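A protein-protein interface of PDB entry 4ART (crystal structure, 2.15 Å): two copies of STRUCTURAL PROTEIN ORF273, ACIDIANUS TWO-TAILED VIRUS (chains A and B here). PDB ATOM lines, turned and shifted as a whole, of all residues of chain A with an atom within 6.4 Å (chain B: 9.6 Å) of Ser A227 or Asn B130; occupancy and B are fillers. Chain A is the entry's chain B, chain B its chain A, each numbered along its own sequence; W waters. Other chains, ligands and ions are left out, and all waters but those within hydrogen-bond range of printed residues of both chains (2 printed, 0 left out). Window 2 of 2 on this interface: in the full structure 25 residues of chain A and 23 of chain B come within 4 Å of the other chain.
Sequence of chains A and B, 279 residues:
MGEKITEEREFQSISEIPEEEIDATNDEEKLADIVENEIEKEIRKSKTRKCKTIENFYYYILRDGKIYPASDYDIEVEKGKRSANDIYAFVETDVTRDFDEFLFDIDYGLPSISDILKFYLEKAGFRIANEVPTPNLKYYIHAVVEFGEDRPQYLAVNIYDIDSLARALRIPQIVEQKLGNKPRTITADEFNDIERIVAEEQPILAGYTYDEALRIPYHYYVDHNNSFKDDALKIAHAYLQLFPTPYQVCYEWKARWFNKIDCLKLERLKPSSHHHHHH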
ATOM      1  N   TYR A 220      21.414 -18.988 -22.896  1.00  0.00           N
ATOM      2  CA  TYR A 220      20.626 -19.662 -21.880  1.00  0.00           C
ATOM      3  C   TYR A 220      19.329 -18.961 -21.580  1.00  0.00           C
ATOM      4  O   TYR A 220      18.291 -19.612 -21.529  1.00  0.00           O
ATOM      5  CB  TYR A 220      21.391 -19.797 -20.562  1.00  0.00           C
ATOM      6  CG  TYR A 220      20.578 -20.431 -19.446  1.00  0.00           C
ATOM      7  CD1 TYR A 220      20.035 -21.706 -19.588  1.00  0.00           C
ATOM      8  CD2 TYR A 220      20.378 -19.767 -18.237  1.00  0.00           C
ATOM      9  CE1 TYR A 220      19.301 -22.300 -18.567  1.00  0.00           C
ATOM     10  CE2 TYR A 220      19.657 -20.358 -17.199  1.00  0.00           C
ATOM     11  CZ  TYR A 220      19.112 -21.622 -17.375  1.00  0.00           C
ATOM     12  OH  TYR A 220      18.367 -22.216 -16.385  1.00  0.00           O
ATOM     13  N   ASN A 225      18.164 -22.103 -24.282  1.00  0.00           N
ATOM     14  CA  ASN A 225      18.963 -23.282 -24.543  1.00  0.00           C
ATOM     15  C   ASN A 225      19.584 -23.719 -23.226  1.00  0.00           C
ATOM     16  O   ASN A 225      20.482 -23.039 -22.726  1.00  0.00           O
ATOM     17  CB  ASN A 225      20.015 -22.984 -25.597  1.00  0.00           C
ATOM     18  CG  ASN A 225      20.755 -24.201 -26.030  1.00  0.00           C
ATOM     19  OD1 ASN A 225      21.304 -24.966 -25.220  1.00  0.00           O
ATOM     20  ND2 ASN A 225      20.724 -24.425 -27.323  1.00  0.00           N
ATOM     21  N   ASN A 226      19.088 -24.836 -22.657  1.00  0.00           N
ATOM     22  CA  ASN A 226      19.504 -25.371 -21.359  1.00  0.00           C
ATOM     23  C   ASN A 226      20.936 -25.842 -21.222  1.00  0.00           C
ATOM     24  O   ASN A 226      21.438 -25.872 -20.098  1.00  0.00           O
ATOM     25  CB  ASN A 226      18.531 -26.433 -20.825  1.00  0.00           C
ATOM     26  CG  ASN A 226      17.586 -25.910 -19.781  1.00  0.00           C
ATOM     27  OD1 ASN A 226      16.772 -25.025 -20.035  1.00  0.00           O
ATOM     28  ND2 ASN A 226      17.667 -26.443 -18.581  1.00  0.00           N
ATOM     29  N   SER A 227      21.588 -26.234 -22.332  1.00  0.00           N
ATOM     30  CA  SER A 227      22.973 -26.722 -22.310  1.00  0.00           C
ATOM     31  C   SER A 227      23.959 -25.665 -21.799  1.00  0.00           C
ATOM     32  O   SER A 227      25.010 -25.997 -21.232  1.00  0.00           O
ATOM     33  CB  SER A 227      23.385 -27.221 -23.690  1.00  0.00           C
ATOM     34  OG  SER A 227      22.636 -28.378 -24.034  1.00  0.00           O
ATOM     35  N   PHE A 228      23.607 -24.399 -21.963  1.00  0.00           N
ATOM     36  CA  PHE A 228      24.462 -23.314 -21.531  1.00  0.00           C
ATOM     37  C   PHE A 228      24.121 -22.769 -20.127  1.00  0.00           C
ATOM     38  O   PHE A 228      24.664 -21.748 -19.733  1.00  0.00           O
ATOM     39  CB  PHE A 228      24.621 -22.286 -22.656  1.00  0.00           C
ATOM     40  CG  PHE A 228      25.337 -22.903 -23.848  1.00  0.00           C
ATOM     41  CD1 PHE A 228      24.666 -23.761 -24.723  1.00  0.00           C
ATOM     42  CD2 PHE A 228      26.687 -22.655 -24.076  1.00  0.00           C
ATOM     43  CE1 PHE A 228      25.335 -24.343 -25.822  1.00  0.00           C
ATOM     44  CE2 PHE A 228      27.350 -23.230 -25.178  1.00  0.00           C
ATOM     45  CZ  PHE A 228      26.670 -24.075 -26.038  1.00  0.00           C
ATOM     46  N   LYS A 229      23.285 -23.515 -19.346  1.00  0.00           N
ATOM     47  CA  LYS A 229      22.904 -23.199 -17.962  1.00  0.00           C
ATOM     48  C   LYS A 229      24.124 -23.000 -17.057  1.00  0.00           C
ATOM     49  O   LYS A 229      24.260 -21.945 -16.438  1.00  0.00           O
ATOM     50  CB  LYS A 229      22.010 -24.312 -17.390  1.00  0.00           C
ATOM     51  CG  LYS A 229      21.490 -24.079 -15.950  1.00  0.00           C
ATOM     52  CD  LYS A 229      20.980 -25.379 -15.333  1.00  0.00           C
ATOM     53  CE  LYS A 229      19.942 -25.163 -14.255  1.00  0.00           C
ATOM     54  NZ  LYS A 229      18.865 -26.221 -14.235  1.00  0.00           N
ATOM     55  N   ASP A 230      24.971 -24.023 -16.935  1.00  0.00           N
ATOM     56  CA  ASP A 230      26.119 -23.979 -16.043  1.00  0.00           C
ATOM     57  C   ASP A 230      26.978 -22.757 -16.242  1.00  0.00           C
ATOM     58  O   ASP A 230      27.233 -22.037 -15.283  1.00  0.00           O
ATOM     59  CB  ASP A 230      26.941 -25.263 -16.174  1.00  0.00           C
ATOM     60  CG  ASP A 230      26.349 -26.477 -15.498  1.00  0.00           C
ATOM     61  OD1 ASP A 230      25.287 -26.338 -14.844  1.00  0.00           O
ATOM     62  OD2 ASP A 230      26.934 -27.574 -15.641  1.00  0.00           O
ATOM     63  N   ASP A 231      27.385 -22.494 -17.500  1.00  0.00           N
ATOM     64  CA  ASP A 231      28.245 -21.360 -17.814  1.00  0.00           C
ATOM     65  C   ASP A 231      27.549 -20.028 -17.649  1.00  0.00           C
ATOM     66  O   ASP A 231      28.169 -19.105 -17.154  1.00  0.00           O
ATOM     67  CB  ASP A 231      28.872 -21.518 -19.224  1.00  0.00           C
ATOM     68  CG  ASP A 231      29.739 -22.768 -19.355  1.00  0.00           C
ATOM     69  OD1 ASP A 231      30.290 -23.220 -18.331  1.00  0.00           O
ATOM     70  OD2 ASP A 231      29.893 -23.268 -20.482  1.00  0.00           O
ATOM     71  N   GLU B  78       9.117 -30.594 -29.784  1.00  0.00           N
ATOM     72  CA  GLU B  78       9.121 -30.999 -28.368  1.00  0.00           C
ATOM     73  C   GLU B  78       7.925 -31.918 -28.021  1.00  0.00           C
ATOM     74  O   GLU B  78       8.009 -32.678 -27.050  1.00  0.00           O
ATOM     75  CB  GLU B  78       9.132 -29.731 -27.471  1.00  0.00           C
ATOM     76  CG  GLU B  78       9.825 -29.909 -26.127  1.00  0.00           C
ATOM     77  CD  GLU B  78       9.627 -28.845 -25.058  1.00  0.00           C
ATOM     78  OE1 GLU B  78       8.894 -27.856 -25.295  1.00  0.00           O
ATOM     79  OE2 GLU B  78      10.199 -29.020 -23.958  1.00  0.00           O
ATOM     80  N   LYS B 118      26.810 -23.805 -34.672  1.00  0.00           N
ATOM     81  CA  LYS B 118      25.795 -24.787 -34.270  1.00  0.00           C
ATOM     82  C   LYS B 118      25.285 -25.536 -35.512  1.00  0.00           C
ATOM     83  O   LYS B 118      25.274 -26.765 -35.531  1.00  0.00           O
ATOM     84  CB  LYS B 118      24.627 -24.088 -33.543  1.00  0.00           C
ATOM     85  CG  LYS B 118      23.410 -24.977 -33.271  1.00  0.00           C
ATOM     86  CD  LYS B 118      22.325 -24.250 -32.479  1.00  0.00           C
ATOM     87  CE  LYS B 118      21.395 -23.411 -33.293  1.00  0.00           C
ATOM     88  NZ  LYS B 118      20.562 -22.537 -32.423  1.00  0.00           N
ATOM     89  N   GLU B 122      26.051 -29.614 -36.324  1.00  0.00           N
ATOM     90  CA  GLU B 122      24.903 -30.517 -36.460  1.00  0.00           C
ATOM     91  C   GLU B 122      24.761 -31.128 -37.837  1.00  0.00           C
ATOM     92  O   GLU B 122      24.362 -32.293 -37.952  1.00  0.00           O
ATOM     93  CB  GLU B 122      23.617 -29.823 -36.032  1.00  0.00           C
ATOM     94  CG  GLU B 122      23.635 -29.627 -34.542  1.00  0.00           C
ATOM     95  CD  GLU B 122      22.561 -28.794 -33.879  1.00  0.00           C
ATOM     96  OE1 GLU B 122      21.668 -28.242 -34.565  1.00  0.00           O
ATOM     97  OE2 GLU B 122      22.585 -28.753 -32.633  1.00  0.00           O
ATOM     98  N   ARG B 127      26.643 -33.578 -32.094  1.00  0.00           N
ATOM     99  CA  ARG B 127      25.498 -33.250 -31.227  1.00  0.00           C
ATOM    100  C   ARG B 127      26.018 -32.349 -30.103  1.00  0.00           C
ATOM    101  O   ARG B 127      27.054 -32.662 -29.530  1.00  0.00           O
ATOM    102  CB  ARG B 127      24.829 -34.529 -30.652  1.00  0.00           C
ATOM    103  CG  ARG B 127      23.756 -35.105 -31.582  1.00  0.00           C
ATOM    104  CD  ARG B 127      22.945 -36.228 -30.940  1.00  0.00           C
ATOM    105  NE  ARG B 127      21.681 -36.486 -31.649  1.00  0.00           N
ATOM    106  CZ  ARG B 127      21.533 -37.342 -32.663  1.00  0.00           C
ATOM    107  NH1 ARG B 127      22.569 -38.042 -33.110  1.00  0.00           N
ATOM    108  NH2 ARG B 127      20.347 -37.497 -33.240  1.00  0.00           N
ATOM    109  N   ILE B 128      25.354 -31.208 -29.844  1.00  0.00           N
ATOM    110  CA  ILE B 128      25.748 -30.268 -28.795  1.00  0.00           C
ATOM    111  C   ILE B 128      24.914 -30.615 -27.568  1.00  0.00           C
ATOM    112  O   ILE B 128      23.682 -30.454 -27.575  1.00  0.00           O
ATOM    113  CB  ILE B 128      25.644 -28.755 -29.247  1.00  0.00           C
ATOM    114  CG1 ILE B 128      26.460 -28.491 -30.523  1.00  0.00           C
ATOM    115  CG2 ILE B 128      26.066 -27.784 -28.139  1.00  0.00           C
ATOM    116  CD1 ILE B 128      26.019 -27.339 -31.336  1.00  0.00           C
ATOM    117  N   ALA B 129      25.593 -31.199 -26.555  1.00  0.00           N
ATOM    118  CA  ALA B 129      25.003 -31.648 -25.296  1.00  0.00           C
ATOM    119  C   ALA B 129      23.630 -32.333 -25.515  1.00  0.00           C
ATOM    120  O   ALA B 129      23.534 -33.193 -26.396  1.00  0.00           O
ATOM    121  CB  ALA B 129      24.922 -30.494 -24.306  1.00  0.00           C
ATOM    122  N   ASN B 130      22.571 -31.928 -24.797  1.00  0.00           N
ATOM    123  CA  ASN B 130      21.267 -32.566 -24.991  1.00  0.00           C
ATOM    124  C   ASN B 130      20.308 -31.819 -25.921  1.00  0.00           C
ATOM    125  O   ASN B 130      19.122 -32.162 -25.979  1.00  0.00           O
ATOM    126  CB  ASN B 130      20.615 -33.010 -23.667  1.00  0.00           C
ATOM    127  CG  ASN B 130      21.395 -34.095 -22.964  1.00  0.00           C
ATOM    128  OD1 ASN B 130      21.215 -35.308 -23.191  1.00  0.00           O
ATOM    129  ND2 ASN B 130      22.335 -33.681 -22.123  1.00  0.00           N
ATOM    130  N   GLU B 131      20.823 -30.860 -26.686  1.00  0.00           N
ATOM    131  CA  GLU B 131      20.025 -30.074 -27.629  1.00  0.00           C
ATOM    132  C   GLU B 131      19.614 -30.805 -28.915  1.00  0.00           C
ATOM    133  O   GLU B 131      20.381 -31.613 -29.441  1.00  0.00           O
ATOM    134  CB  GLU B 131      20.684 -28.720 -27.920  1.00  0.00           C
ATOM    135  CG  GLU B 131      20.777 -27.810 -26.701  1.00  0.00           C
ATOM    136  CD  GLU B 131      19.553 -27.710 -25.802  1.00  0.00           C
ATOM    137  OE1 GLU B 131      18.521 -27.170 -26.266  1.00  0.00           O
ATOM    138  OE2 GLU B 131      19.624 -28.174 -24.639  1.00  0.00           O
ATOM    139  N   VAL B 132      18.397 -30.493 -29.417  1.00  0.00           N
ATOM    140  CA  VAL B 132      17.758 -31.113 -30.580  1.00  0.00           C
ATOM    141  C   VAL B 132      18.442 -30.620 -31.851  1.00  0.00           C
ATOM    142  O   VAL B 132      18.428 -29.423 -32.126  1.00  0.00           O
ATOM    143  CB  VAL B 132      16.200 -30.968 -30.599  1.00  0.00           C
ATOM    144  CG1 VAL B 132      15.583 -31.703 -31.789  1.00  0.00           C
ATOM    145  CG2 VAL B 132      15.579 -31.461 -29.291  1.00  0.00           C
ATOM    146  N   PRO B 133      19.099 -31.528 -32.601  1.00  0.00           N
ATOM    147  CA  PRO B 133      19.824 -31.088 -33.801  1.00  0.00           C
ATOM    148  C   PRO B 133      18.922 -30.747 -34.994  1.00  0.00           C
ATOM    149  O   PRO B 133      17.812 -31.275 -35.110  1.00  0.00           O
ATOM    150  CB  PRO B 133      20.754 -32.276 -34.088  1.00  0.00           C
ATOM    151  CG  PRO B 133      20.007 -33.466 -33.589  1.00  0.00           C
ATOM    152  CD  PRO B 133      19.255 -32.985 -32.374  1.00  0.00           C
ATOM    153  N   THR B 185      28.775 -36.333 -29.417  1.00  0.00           N
ATOM    154  CA  THR B 185      28.146 -35.293 -28.623  1.00  0.00           C
ATOM    155  C   THR B 185      29.286 -34.497 -27.994  1.00  0.00           C
ATOM    156  O   THR B 185      30.172 -35.087 -27.371  1.00  0.00           O
ATOM    157  CB  THR B 185      27.216 -35.888 -27.551  1.00  0.00           C
ATOM    158  OG1 THR B 185      26.322 -36.819 -28.162  1.00  0.00           O
ATOM    159  CG2 THR B 185      26.425 -34.805 -26.805  1.00  0.00           C
ATOM    160  N   ILE B 186      29.266 -33.179 -28.149  1.00  0.00           N
ATOM    161  CA  ILE B 186      30.268 -32.295 -27.543  1.00  0.00           C
ATOM    162  C   ILE B 186      29.656 -31.578 -26.333  1.00  0.00           C
ATOM    163  O   ILE B 186      28.432 -31.437 -26.253  1.00  0.00           O
ATOM    164  CB  ILE B 186      30.870 -31.314 -28.594  1.00  0.00           C
ATOM    165  CG1 ILE B 186      29.845 -30.266 -29.082  1.00  0.00           C
ATOM    166  CG2 ILE B 186      31.477 -32.093 -29.753  1.00  0.00           C
ATOM    167  CD1 ILE B 186      30.424 -28.960 -29.496  1.00  0.00           C
ATOM    168  N   THR B 187      30.492 -31.120 -25.404  1.00  0.00           N
ATOM    169  CA  THR B 187      30.012 -30.379 -24.236  1.00  0.00           C
ATOM    170  C   THR B 187      29.807 -28.902 -24.640  1.00  0.00           C
ATOM    171  O   THR B 187      30.301 -28.469 -25.695  1.00  0.00           O
ATOM    172  CB  THR B 187      31.033 -30.448 -23.079  1.00  0.00           C
ATOM    173  OG1 THR B 187      32.224 -29.789 -23.499  1.00  0.00           O
ATOM    174  CG2 THR B 187      31.349 -31.879 -22.626  1.00  0.00           C
ATOM    175  N   ALA B 188      29.139 -28.120 -23.764  1.00  0.00           N
ATOM    176  CA  ALA B 188      28.950 -26.677 -23.938  1.00  0.00           C
ATOM    177  C   ALA B 188      30.330 -25.992 -23.909  1.00  0.00           C
ATOM    178  O   ALA B 188      30.574 -25.056 -24.671  1.00  0.00           O
ATOM    179  CB  ALA B 188      28.067 -26.129 -22.829  1.00  0.00           C
ATOM    180  N   ASP B 189      31.240 -26.497 -23.042  1.00  0.00           N
ATOM    181  CA  ASP B 189      32.605 -25.989 -22.918  1.00  0.00           C
ATOM    182  C   ASP B 189      33.376 -26.129 -24.219  1.00  0.00           C
ATOM    183  O   ASP B 189      34.054 -25.181 -24.617  1.00  0.00           O
ATOM    184  CB  ASP B 189      33.344 -26.640 -21.757  1.00  0.00           C
ATOM    185  CG  ASP B 189      32.766 -26.238 -20.410  1.00  0.00           C
ATOM    186  OD1 ASP B 189      32.413 -25.039 -20.241  1.00  0.00           O
ATOM    187  OD2 ASP B 189      32.602 -27.127 -19.548  1.00  0.00           O
ATOM    188  N   GLU B 190      33.222 -27.278 -24.906  1.00  0.00           N
ATOM    189  CA  GLU B 190      33.865 -27.549 -26.204  1.00  0.00           C
ATOM    190  C   GLU B 190      33.328 -26.635 -27.283  1.00  0.00           C
ATOM    191  O   GLU B 190      34.085 -26.154 -28.122  1.00  0.00           O
ATOM    192  CB  GLU B 190      33.710 -29.013 -26.595  1.00  0.00           C
ATOM    193  CG  GLU B 190      34.603 -29.918 -25.758  1.00  0.00           C
ATOM    194  CD  GLU B 190      34.527 -31.393 -26.109  1.00  0.00           C
ATOM    195  OE1 GLU B 190      33.400 -31.922 -26.253  1.00  0.00           O
ATOM    196  OE2 GLU B 190      35.601 -32.028 -26.206  1.00  0.00           O
ATOM    197  N   PHE B 191      32.018 -26.391 -27.266  1.00  0.00           N
ATOM    198  CA  PHE B 191      31.381 -25.479 -28.199  1.00  0.00           C
ATOM    199  C   PHE B 191      31.978 -24.079 -27.993  1.00  0.00           C
ATOM    200  O   PHE B 191      32.382 -23.439 -28.960  1.00  0.00           O
ATOM    201  CB  PHE B 191      29.857 -25.465 -27.986  1.00  0.00           C
ATOM    202  CG  PHE B 191      29.122 -24.564 -28.934  1.00  0.00           C
ATOM    203  CD1 PHE B 191      28.951 -23.212 -28.647  1.00  0.00           C
ATOM    204  CD2 PHE B 191      28.585 -25.068 -30.093  1.00  0.00           C
ATOM    205  CE1 PHE B 191      28.299 -22.380 -29.523  1.00  0.00           C
ATOM    206  CE2 PHE B 191      27.927 -24.234 -30.966  1.00  0.00           C
ATOM    207  CZ  PHE B 191      27.797 -22.892 -30.672  1.00  0.00           C
ATOM    208  N   ASN B 192      32.046 -23.623 -26.724  1.00  0.00           N
ATOM    209  CA  ASN B 192      32.591 -22.319 -26.346  1.00  0.00           C
ATOM    210  C   ASN B 192      34.046 -22.123 -26.753  1.00  0.00           C
ATOM    211  O   ASN B 192      34.391 -21.046 -27.252  1.00  0.00           O
ATOM    212  CB  ASN B 192      32.349 -22.036 -24.853  1.00  0.00           C
ATOM    213  CG  ASN B 192      30.889 -21.846 -24.507  1.00  0.00           C
ATOM    214  OD1 ASN B 192      30.056 -21.455 -25.346  1.00  0.00           O
ATOM    215  ND2 ASN B 192      30.550 -22.122 -23.261  1.00  0.00           N
HETATM  216  O   HOH W   1      17.007 -26.508 -23.774  1.00  0.00           O
HETATM  217  O   HOH W   2      32.966 -22.746 -21.537  1.00  0.00           O
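The backbone carbonyl oxygen (O) of Ile B186 is in hydrogen-bond range of the backbone NH (N) of Ala B129 (2.9 Å).
The side-chain hydroxyl of Thr B187 lies close to the backbone NH of Asp B189 (3.5 Å).
The backbone carbonyl oxygen of Ala B188 lies close to the side-chain amide nitrogen of Asn B192 (3.3 Å).
The side-chain amide oxygen of Asn A225 sits at hydrogen-bond distance from the backbone NH of Ser A227, 3.2 Å away.
Among the printed residues, pairs that only touch across the chains: Asn A225 with Glu B131 (3.2 Å), Asn A226 with Glu B131 (3.9 Å), Ser A227 with Ala B129 (3.1 Å), Ser A227 with Asn B130 (3.6 Å), Ser A227 with Ala B188 (3.5 Å), Phe A228 with Ala B188 (3.7 Å), Phe A228 with Phe B191 (3.6 Å) and Phe A228 with Asn B192 (3.2 Å).
Printed residues of chain B that touch a printed residue of chain A: Ala B129, Asn B130, Glu B131, Ala B188, Asp B189, Phe B191 and Asn B192.
Hydrophobic or aromatic side chains of chain B that line the printed part of chain A: Ala B129, Ala B188 and Phe B191.
Among the printed residues, no Asp or Glu carboxylate lies within 4 Å of a Lys or Arg side-chain nitrogen of the other chain.
Water W2 lies within hydrogen-bond range of the side-chain carboxylate (OD1) of Asp B189 (2.7 Å), the side-chain amide nitrogen (ND2) of Asn B192 (3.0 Å) and the side-chain carboxylate (OD2) of Asp A231 (3.3 Å).
Water W1 bridges N of Asn A226 and OE1 of Glu B131.
No position is printed for both chains.
OG of Ser A227 is in hydrogen-bond range of OE2 of Glu B131 (3.1 Å).
The side-chain carboxylate (OD2) of Asp A231 is in hydrogen-bond range of the side-chain amide nitrogen (ND2) of Asn B192, at 3.1 Å.
The side-chain carboxylate of Asp B189 sits close to the side-chain carboxylate of Asp A231 (3.1 Å).
Of chain A, only Ser A227 comes within 4 Å of Asn B130.
Of chain B, only Glu B131 comes within 4 Å of Asn A226.
Of chain B, only Ala B188 (3.7 Å), Phe B191 (3.6 Å) and Asn B192 (3.2 Å) come within 4 Å of Phe A228.
Of the printed residues of chain A, Asp B189 touches Asp A231 (3.1 Å).
Of the printed residues of chain B, Asp A231 touches Asp B189 (3.1 Å) and Asn B192 (3.1 Å).
The nearest residue of chain B that does not touch Ser A227 is Ile B128 (4.2 Å).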
